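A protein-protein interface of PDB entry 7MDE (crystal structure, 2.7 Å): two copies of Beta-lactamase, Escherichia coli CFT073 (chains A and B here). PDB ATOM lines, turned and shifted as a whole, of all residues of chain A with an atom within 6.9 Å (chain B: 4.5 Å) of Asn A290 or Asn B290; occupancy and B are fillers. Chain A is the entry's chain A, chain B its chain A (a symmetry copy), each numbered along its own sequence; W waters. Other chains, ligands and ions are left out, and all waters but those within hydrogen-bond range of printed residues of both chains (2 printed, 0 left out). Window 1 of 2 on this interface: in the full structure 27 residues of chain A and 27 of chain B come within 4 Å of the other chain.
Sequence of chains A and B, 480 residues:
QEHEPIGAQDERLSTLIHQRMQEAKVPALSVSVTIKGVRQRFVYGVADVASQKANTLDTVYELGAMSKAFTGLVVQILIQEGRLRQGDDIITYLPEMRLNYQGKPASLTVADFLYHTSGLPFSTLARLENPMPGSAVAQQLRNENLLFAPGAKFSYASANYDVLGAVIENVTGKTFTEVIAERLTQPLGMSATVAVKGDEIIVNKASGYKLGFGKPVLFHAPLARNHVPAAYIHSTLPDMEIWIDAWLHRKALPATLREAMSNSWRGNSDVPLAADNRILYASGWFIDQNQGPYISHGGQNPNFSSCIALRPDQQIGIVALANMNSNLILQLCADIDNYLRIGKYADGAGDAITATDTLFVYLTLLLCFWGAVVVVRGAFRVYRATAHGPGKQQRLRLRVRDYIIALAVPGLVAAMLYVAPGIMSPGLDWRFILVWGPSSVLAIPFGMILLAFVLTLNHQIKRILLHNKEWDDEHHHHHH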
ATOM      1  N   LEU A 273      38.032 -32.632  -3.249  1.00  0.00           N
ATOM      2  CA  LEU A 273      37.154 -31.645  -2.651  1.00  0.00           C
ATOM      3  C   LEU A 273      37.778 -31.141  -1.362  1.00  0.00           C
ATOM      4  O   LEU A 273      38.456 -31.893  -0.651  1.00  0.00           O
ATOM      5  CB  LEU A 273      35.782 -32.245  -2.371  1.00  0.00           C
ATOM      6  CG  LEU A 273      35.132 -32.954  -3.539  1.00  0.00           C
ATOM      7  CD1 LEU A 273      33.961 -33.800  -3.052  1.00  0.00           C
ATOM      8  CD2 LEU A 273      34.689 -31.937  -4.586  1.00  0.00           C
ATOM      9  N   ASN A 277      34.011 -27.402   0.921  1.00  0.00           N
ATOM     10  CA  ASN A 277      33.471 -27.208  -0.412  1.00  0.00           C
ATOM     11  C   ASN A 277      33.532 -28.545  -1.154  1.00  0.00           C
ATOM     12  O   ASN A 277      34.594 -28.947  -1.651  1.00  0.00           O
ATOM     13  CB  ASN A 277      34.233 -26.119  -1.146  1.00  0.00           C
ATOM     14  CG  ASN A 277      33.419 -25.503  -2.271  1.00  0.00           C
ATOM     15  OD1 ASN A 277      32.462 -26.113  -2.775  1.00  0.00           O
ATOM     16  ND2 ASN A 277      33.782 -24.285  -2.665  1.00  0.00           N
ATOM     17  N   ARG A 278      32.381 -29.209  -1.232  1.00  0.00           N
ATOM     18  CA  ARG A 278      32.226 -30.403  -2.050  1.00  0.00           C
ATOM     19  C   ARG A 278      31.312 -30.158  -3.259  1.00  0.00           C
ATOM     20  O   ARG A 278      30.739 -31.113  -3.805  1.00  0.00           O
ATOM     21  CB  ARG A 278      31.719 -31.548  -1.169  1.00  0.00           C
ATOM     22  CG  ARG A 278      32.582 -31.732   0.093  1.00  0.00           C
ATOM     23  CD  ARG A 278      31.978 -32.711   1.083  1.00  0.00           C
ATOM     24  NE  ARG A 278      31.989 -34.113   0.665  1.00  0.00           N
ATOM     25  CZ  ARG A 278      32.978 -34.980   0.886  1.00  0.00           C
ATOM     26  NH1 ARG A 278      34.135 -34.596   1.401  1.00  0.00           N
ATOM     27  NH2 ARG A 278      32.795 -36.266   0.586  1.00  0.00           N
ATOM     28  N   ILE A 279      31.171 -28.890  -3.678  1.00  0.00           N
ATOM     29  CA  ILE A 279      30.349 -28.523  -4.830  1.00  0.00           C
ATOM     30  C   ILE A 279      31.065 -28.913  -6.118  1.00  0.00           C
ATOM     31  O   ILE A 279      32.291 -28.766  -6.242  1.00  0.00           O
ATOM     32  CB  ILE A 279      30.042 -27.012  -4.816  1.00  0.00           C
ATOM     33  CG1 ILE A 279      29.210 -26.615  -3.605  1.00  0.00           C
ATOM     34  CG2 ILE A 279      29.334 -26.573  -6.086  1.00  0.00           C
ATOM     35  CD1 ILE A 279      29.283 -25.133  -3.330  1.00  0.00           C
ATOM     36  N   LEU A 280      30.294 -29.384  -7.094  1.00  0.00           N
ATOM     37  CA  LEU A 280      30.813 -29.876  -8.363  1.00  0.00           C
ATOM     38  C   LEU A 280      30.538 -28.887  -9.498  1.00  0.00           C
ATOM     39  O   LEU A 280      29.546 -28.151  -9.495  1.00  0.00           O
ATOM     40  CB  LEU A 280      30.188 -31.233  -8.710  1.00  0.00           C
ATOM     41  CG  LEU A 280      30.281 -32.379  -7.702  1.00  0.00           C
ATOM     42  CD1 LEU A 280      29.764 -33.693  -8.308  1.00  0.00           C
ATOM     43  CD2 LEU A 280      31.709 -32.536  -7.188  1.00  0.00           C
ATOM     44  N   ILE A 287      27.030 -27.182  -9.331  1.00  0.00           N
ATOM     45  CA  ILE A 287      26.001 -28.078  -8.816  1.00  0.00           C
ATOM     46  C   ILE A 287      26.237 -28.264  -7.333  1.00  0.00           C
ATOM     47  O   ILE A 287      27.283 -28.793  -6.933  1.00  0.00           O
ATOM     48  CB  ILE A 287      26.026 -29.444  -9.500  1.00  0.00           C
ATOM     49  CG1 ILE A 287      26.333 -29.298 -11.007  1.00  0.00           C
ATOM     50  CG2 ILE A 287      24.755 -30.199  -9.150  1.00  0.00           C
ATOM     51  CD1 ILE A 287      25.199 -28.853 -11.873  1.00  0.00           C
ATOM     52  N   ASP A 288      25.242 -27.871  -6.531  1.00  0.00           N
ATOM     53  CA  ASP A 288      25.247 -27.989  -5.077  1.00  0.00           C
ATOM     54  C   ASP A 288      23.994 -28.745  -4.655  1.00  0.00           C
ATOM     55  O   ASP A 288      22.880 -28.286  -4.917  1.00  0.00           O
ATOM     56  CB  ASP A 288      25.279 -26.601  -4.428  1.00  0.00           C
ATOM     57  CG  ASP A 288      25.572 -26.644  -2.939  1.00  0.00           C
ATOM     58  OD1 ASP A 288      25.328 -27.699  -2.290  1.00  0.00           O
ATOM     59  OD2 ASP A 288      26.039 -25.597  -2.418  1.00  0.00           O
ATOM     60  N   GLN A 289      24.170 -29.887  -3.994  1.00  0.00           N
ATOM     61  CA  GLN A 289      23.039 -30.683  -3.523  1.00  0.00           C
ATOM     62  C   GLN A 289      22.489 -30.234  -2.170  1.00  0.00           C
ATOM     63  O   GLN A 289      21.430 -30.723  -1.765  1.00  0.00           O
ATOM     64  CB  GLN A 289      23.439 -32.156  -3.428  1.00  0.00           C
ATOM     65  CG  GLN A 289      23.915 -32.725  -4.731  1.00  0.00           C
ATOM     66  CD  GLN A 289      22.782 -32.926  -5.718  1.00  0.00           C
ATOM     67  OE1 GLN A 289      21.643 -33.173  -5.320  1.00  0.00           O
ATOM     68  NE2 GLN A 289      23.088 -32.821  -7.017  1.00  0.00           N
ATOM     69  N   ASN A 290      23.186 -29.335  -1.473  1.00  0.00           N
ATOM     70  CA  ASN A 290      22.778 -28.843  -0.160  1.00  0.00           C
ATOM     71  C   ASN A 290      21.592 -27.891  -0.284  1.00  0.00           C
ATOM     72  O   ASN A 290      21.709 -26.837  -0.924  1.00  0.00           O
ATOM     73  CB  ASN A 290      23.941 -28.101   0.500  1.00  0.00           C
ATOM     74  CG  ASN A 290      24.982 -29.020   1.100  1.00  0.00           C
ATOM     75  OD1 ASN A 290      24.668 -30.111   1.597  1.00  0.00           O
ATOM     76  ND2 ASN A 290      26.240 -28.571   1.077  1.00  0.00           N
ATOM     77  N   GLN A 291      20.486 -28.201   0.402  1.00  0.00           N
ATOM     78  CA  GLN A 291      19.244 -27.434   0.262  1.00  0.00           C
ATOM     79  C   GLN A 291      18.912 -27.287  -1.213  1.00  0.00           C
ATOM     80  O   GLN A 291      18.609 -26.188  -1.707  1.00  0.00           O
ATOM     81  CB  GLN A 291      19.326 -26.048   0.926  1.00  0.00           C
ATOM     82  CG  GLN A 291      19.457 -26.033   2.442  1.00  0.00           C
ATOM     83  CD  GLN A 291      18.275 -26.677   3.132  1.00  0.00           C
ATOM     84  OE1 GLN A 291      17.233 -26.037   3.332  1.00  0.00           O
ATOM     85  NE2 GLN A 291      18.419 -27.953   3.486  1.00  0.00           N
ATOM     86  N   GLY A 292      19.015 -28.416  -1.925  1.00  0.00           N
ATOM     87  CA  GLY A 292      19.070 -28.400  -3.368  1.00  0.00           C
ATOM     88  C   GLY A 292      18.261 -29.481  -4.059  1.00  0.00           C
ATOM     89  O   GLY A 292      17.326 -30.052  -3.489  1.00  0.00           O
ATOM     90  N   PRO A 293      18.613 -29.789  -5.322  1.00  0.00           N
ATOM     91  CA  PRO A 293      19.745 -29.231  -6.068  1.00  0.00           C
ATOM     92  C   PRO A 293      19.621 -27.729  -6.365  1.00  0.00           C
ATOM     93  O   PRO A 293      18.541 -27.194  -6.631  1.00  0.00           O
ATOM     94  CB  PRO A 293      19.733 -30.032  -7.383  1.00  0.00           C
ATOM     95  CG  PRO A 293      18.916 -31.230  -7.109  1.00  0.00           C
ATOM     96  CD  PRO A 293      17.884 -30.787  -6.123  1.00  0.00           C
ATOM     97  N   TYR A 294      20.764 -27.060  -6.298  1.00  0.00           N
ATOM     98  CA  TYR A 294      20.867 -25.620  -6.472  1.00  0.00           C
ATOM     99  C   TYR A 294      21.907 -25.427  -7.563  1.00  0.00           C
ATOM    100  O   TYR A 294      23.106 -25.646  -7.332  1.00  0.00           O
ATOM    101  CB  TYR A 294      21.260 -24.951  -5.153  1.00  0.00           C
ATOM    102  CG  TYR A 294      21.399 -23.460  -5.199  1.00  0.00           C
ATOM    103  CD1 TYR A 294      20.276 -22.638  -5.124  1.00  0.00           C
ATOM    104  CD2 TYR A 294      22.653 -22.862  -5.264  1.00  0.00           C
ATOM    105  CE1 TYR A 294      20.394 -21.249  -5.152  1.00  0.00           C
ATOM    106  CE2 TYR A 294      22.791 -21.476  -5.302  1.00  0.00           C
ATOM    107  CZ  TYR A 294      21.652 -20.679  -5.251  1.00  0.00           C
ATOM    108  OH  TYR A 294      21.772 -19.313  -5.270  1.00  0.00           O
ATOM    109  N   ARG A 311      16.591 -23.811  -8.853  1.00  0.00           N
ATOM    110  CA  ARG A 311      16.234 -24.815  -7.861  1.00  0.00           C
ATOM    111  C   ARG A 311      15.141 -25.646  -8.514  1.00  0.00           C
ATOM    112  O   ARG A 311      13.947 -25.475  -8.215  1.00  0.00           O
ATOM    113  CB  ARG A 311      15.787 -24.158  -6.557  1.00  0.00           C
ATOM    114  CG  ARG A 311      16.079 -24.984  -5.308  1.00  0.00           C
ATOM    115  CD  ARG A 311      16.692 -24.154  -4.166  1.00  0.00           C
ATOM    116  NE  ARG A 311      15.906 -22.982  -3.781  1.00  0.00           N
ATOM    117  CZ  ARG A 311      14.809 -23.012  -3.033  1.00  0.00           C
ATOM    118  NH1 ARG A 311      14.286 -24.156  -2.616  1.00  0.00           N
ATOM    119  NH2 ARG A 311      14.223 -21.866  -2.693  1.00  0.00           N
ATOM    120  N   ARG B 278      26.213 -23.850   1.419  1.00  0.00           N
ATOM    121  CA  ARG B 278      24.901 -24.200   1.942  1.00  0.00           C
ATOM    122  C   ARG B 278      24.976 -25.326   2.982  1.00  0.00           C
ATOM    123  O   ARG B 278      23.978 -26.024   3.211  1.00  0.00           O
ATOM    124  CB  ARG B 278      23.978 -24.558   0.773  1.00  0.00           C
ATOM    125  CG  ARG B 278      23.975 -23.469  -0.316  1.00  0.00           C
ATOM    126  CD  ARG B 278      23.243 -23.896  -1.575  1.00  0.00           C
ATOM    127  NE  ARG B 278      21.790 -24.010  -1.447  1.00  0.00           N
ATOM    128  CZ  ARG B 278      20.914 -23.023  -1.645  1.00  0.00           C
ATOM    129  NH1 ARG B 278      21.309 -21.776  -1.848  1.00  0.00           N
ATOM    130  NH2 ARG B 278      19.611 -23.301  -1.645  1.00  0.00           N
ATOM    131  N   ILE B 279      26.150 -25.509   3.608  1.00  0.00           N
ATOM    132  CA  ILE B 279      26.349 -26.530   4.635  1.00  0.00           C
ATOM    133  C   ILE B 279      25.678 -26.094   5.932  1.00  0.00           C
ATOM    134  O   ILE B 279      25.715 -24.913   6.310  1.00  0.00           O
ATOM    135  CB  ILE B 279      27.854 -26.781   4.862  1.00  0.00           C
ATOM    136  CG1 ILE B 279      28.526 -27.346   3.619  1.00  0.00           C
ATOM    137  CG2 ILE B 279      28.094 -27.713   6.038  1.00  0.00           C
ATOM    138  CD1 ILE B 279      30.025 -27.176   3.660  1.00  0.00           C
ATOM    139  N   ASP B 288      27.017 -31.850   5.443  1.00  0.00           N
ATOM    140  CA  ASP B 288      27.174 -31.562   4.021  1.00  0.00           C
ATOM    141  C   ASP B 288      26.597 -32.730   3.232  1.00  0.00           C
ATOM    142  O   ASP B 288      27.074 -33.859   3.366  1.00  0.00           O
ATOM    143  CB  ASP B 288      28.653 -31.361   3.677  1.00  0.00           C
ATOM    144  CG  ASP B 288      28.870 -30.781   2.290  1.00  0.00           C
ATOM    145  OD1 ASP B 288      27.975 -30.925   1.412  1.00  0.00           O
ATOM    146  OD2 ASP B 288      29.962 -30.188   2.083  1.00  0.00           O
ATOM    147  N   GLN B 289      25.590 -32.462   2.404  1.00  0.00           N
ATOM    148  CA  GLN B 289      24.976 -33.501   1.581  1.00  0.00           C
ATOM    149  C   GLN B 289      25.707 -33.760   0.265  1.00  0.00           C
ATOM    150  O   GLN B 289      25.375 -34.732  -0.419  1.00  0.00           O
ATOM    151  CB  GLN B 289      23.523 -33.135   1.275  1.00  0.00           C
ATOM    152  CG  GLN B 289      22.689 -32.943   2.506  1.00  0.00           C
ATOM    153  CD  GLN B 289      22.383 -34.253   3.204  1.00  0.00           C
ATOM    154  OE1 GLN B 289      22.294 -35.299   2.558  1.00  0.00           O
ATOM    155  NE2 GLN B 289      22.223 -34.207   4.532  1.00  0.00           N
ATOM    156  N   ASN B 290      26.671 -32.912  -0.098  1.00  0.00           N
ATOM    157  CA  ASN B 290      27.426 -33.038  -1.341  1.00  0.00           C
ATOM    158  C   ASN B 290      28.417 -34.195  -1.256  1.00  0.00           C
ATOM    159  O   ASN B 290      29.322 -34.176  -0.411  1.00  0.00           O
ATOM    160  CB  ASN B 290      28.198 -31.746  -1.612  1.00  0.00           C
ATOM    161  CG  ASN B 290      27.339 -30.636  -2.175  1.00  0.00           C
ATOM    162  OD1 ASN B 290      26.385 -30.879  -2.927  1.00  0.00           O
ATOM    163  ND2 ASN B 290      27.689 -29.394  -1.829  1.00  0.00           N
ATOM    164  N   GLN B 291      28.317 -35.154  -2.185  1.00  0.00           N
ATOM    165  CA  GLN B 291      29.127 -36.375  -2.132  1.00  0.00           C
ATOM    166  C   GLN B 291      29.017 -36.987  -0.745  1.00  0.00           C
ATOM    167  O   GLN B 291      30.022 -37.348  -0.110  1.00  0.00           O
ATOM    168  CB  GLN B 291      30.604 -36.122  -2.482  1.00  0.00           C
ATOM    169  CG  GLN B 291      30.893 -35.694  -3.913  1.00  0.00           C
ATOM    170  CD  GLN B 291      30.473 -36.736  -4.926  1.00  0.00           C
ATOM    171  OE1 GLN B 291      31.208 -37.699  -5.187  1.00  0.00           O
ATOM    172  NE2 GLN B 291      29.279 -36.564  -5.491  1.00  0.00           N
ATOM    173  N   GLY B 292      27.770 -37.061  -0.264  1.00  0.00           N
ATOM    174  CA  GLY B 292      27.512 -37.291   1.139  1.00  0.00           C
ATOM    175  C   GLY B 292      26.379 -38.252   1.439  1.00  0.00           C
ATOM    176  O   GLY B 292      25.989 -39.073   0.602  1.00  0.00           O
HETATM  177  O   HOH W   1      29.751 -28.260   0.090  1.00  0.00           O
HETATM  178  O   HOH W   2      27.570 -26.139  -0.159  1.00  0.00           O
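Of the 14 printed residues of chain A, 9 touch a printed residue of chain B.
Printed residues of chain A that touch a printed residue of chain B: Leu A273, Arg A278, Ile A279, Asp A288, Gln A289, Asn A290, Gln A291, Tyr A294 and Arg A311.
Hydrophobic or aromatic side chains of chain A within 4 Å of the printed part of chain B: Leu A273, Ile A279 and Tyr A294.
Among the printed residues, 16 pairs touch across the chains.
OD1 of Asp A288 lies within hydrogen-bond range of ND2 of Asn B290 (2.9 Å).
OD1 of Asn B290 sits at hydrogen-bond distance from N of Gln A289 (2.7 Å).
The side-chain amide nitrogen of Asn A290 lies close to the side-chain amide nitrogen of Asn B290, at 3.3 Å.
O of Gln A291 sits at hydrogen-bond distance from NH2 of Arg B278, at 3.1 Å.
O of Asn A290 is in hydrogen-bond range of NE of Arg B278.
NE of Arg A278 is in hydrogen-bond range of O of Asn B290.
The backbone carbonyl oxygen of Gln B291 lies within hydrogen-bond range of the guanidinium group of Arg A278.
The side-chain carboxylate (OD1) of Asp B288 sits at hydrogen-bond distance from the side-chain amide nitrogen (ND2) of Asn A290 (2.9 Å).
N of Gln B289 sits at hydrogen-bond distance from OD1 of Asn A290 (2.7 Å).
Water W2 lies within hydrogen-bond range of the side-chain carboxylate of Asp A288 (2.8 Å), the side-chain amide nitrogen of Asn A290 (3.0 Å) and the backbone NH of Arg B278 (3.1 Å).
Water W1 lies within hydrogen-bond range of the side-chain carboxylate of Asp B288 (2.8 Å), the side-chain amide nitrogen of Asn B290 (3.0 Å) and the backbone NH of Arg A278 (3.1 Å).
The backbone NH (N) of Asn A290 sits at hydrogen-bond distance from the side-chain carboxylate (OD1) of Asp A288 (2.8 Å).
The side-chain amide oxygen of Asn A277 sits at hydrogen-bond distance from the backbone NH of Ile A279.
The backbone NH (N) of Tyr A294 lies within hydrogen-bond range of the backbone carbonyl oxygen (O) of Asp A288, 2.8 Å away.
The backbone NH of Asn B290 lies within hydrogen-bond range of the side-chain carboxylate of Asp B288 (2.8 Å).
Printed residues of chain B within 4 Å of Leu A273: Gln B291 (3.7 Å).
Asn A277 touches none of the printed residues of chain B.
Of the printed residues of chain B, Ile A279 touches Asn B290 (3.6 Å).
Of chain B, only Arg B278, Ile B279, Asp B288, Gln B289 and Asn B290 come within 4 Å of Asn A290.
Of the printed residues of chain B, Gln A291 touches Arg B278.
Of the printed residues of chain B, Tyr A294 touches Arg B278.
Of the printed residues of chain A, Arg B278 touches Asp A288, Asn A290, Gln A291, Tyr A294 and Arg A311.
Gly B292 touches none of the printed residues of chain A.
Among the printed residues, merely in contact across the chains: Asp A288 with Arg B278, Arg A278 with Asp B288, Tyr A294 with Arg B278, Asn A290 with Ile B279, Ile A279 with Asn B290, Leu A273 with Gln B291 and Arg A311 with Arg B278.
Arg A278 touches Asn B290, and with the chains exchanged Asn A290 touches Arg B278.
Ile A279 touches Asn B290, and with the chains exchanged Asn A290 touches Ile B279.
Asp A288 touches Asn B290, and with the chains exchanged Asn A290 touches Asp B288.
Asn B290 touches its own counterpart, Asn A290.
Of the 16 pairs that touch across the chains among the printed residues, 13 have their exchanged pair printed and touching as well.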
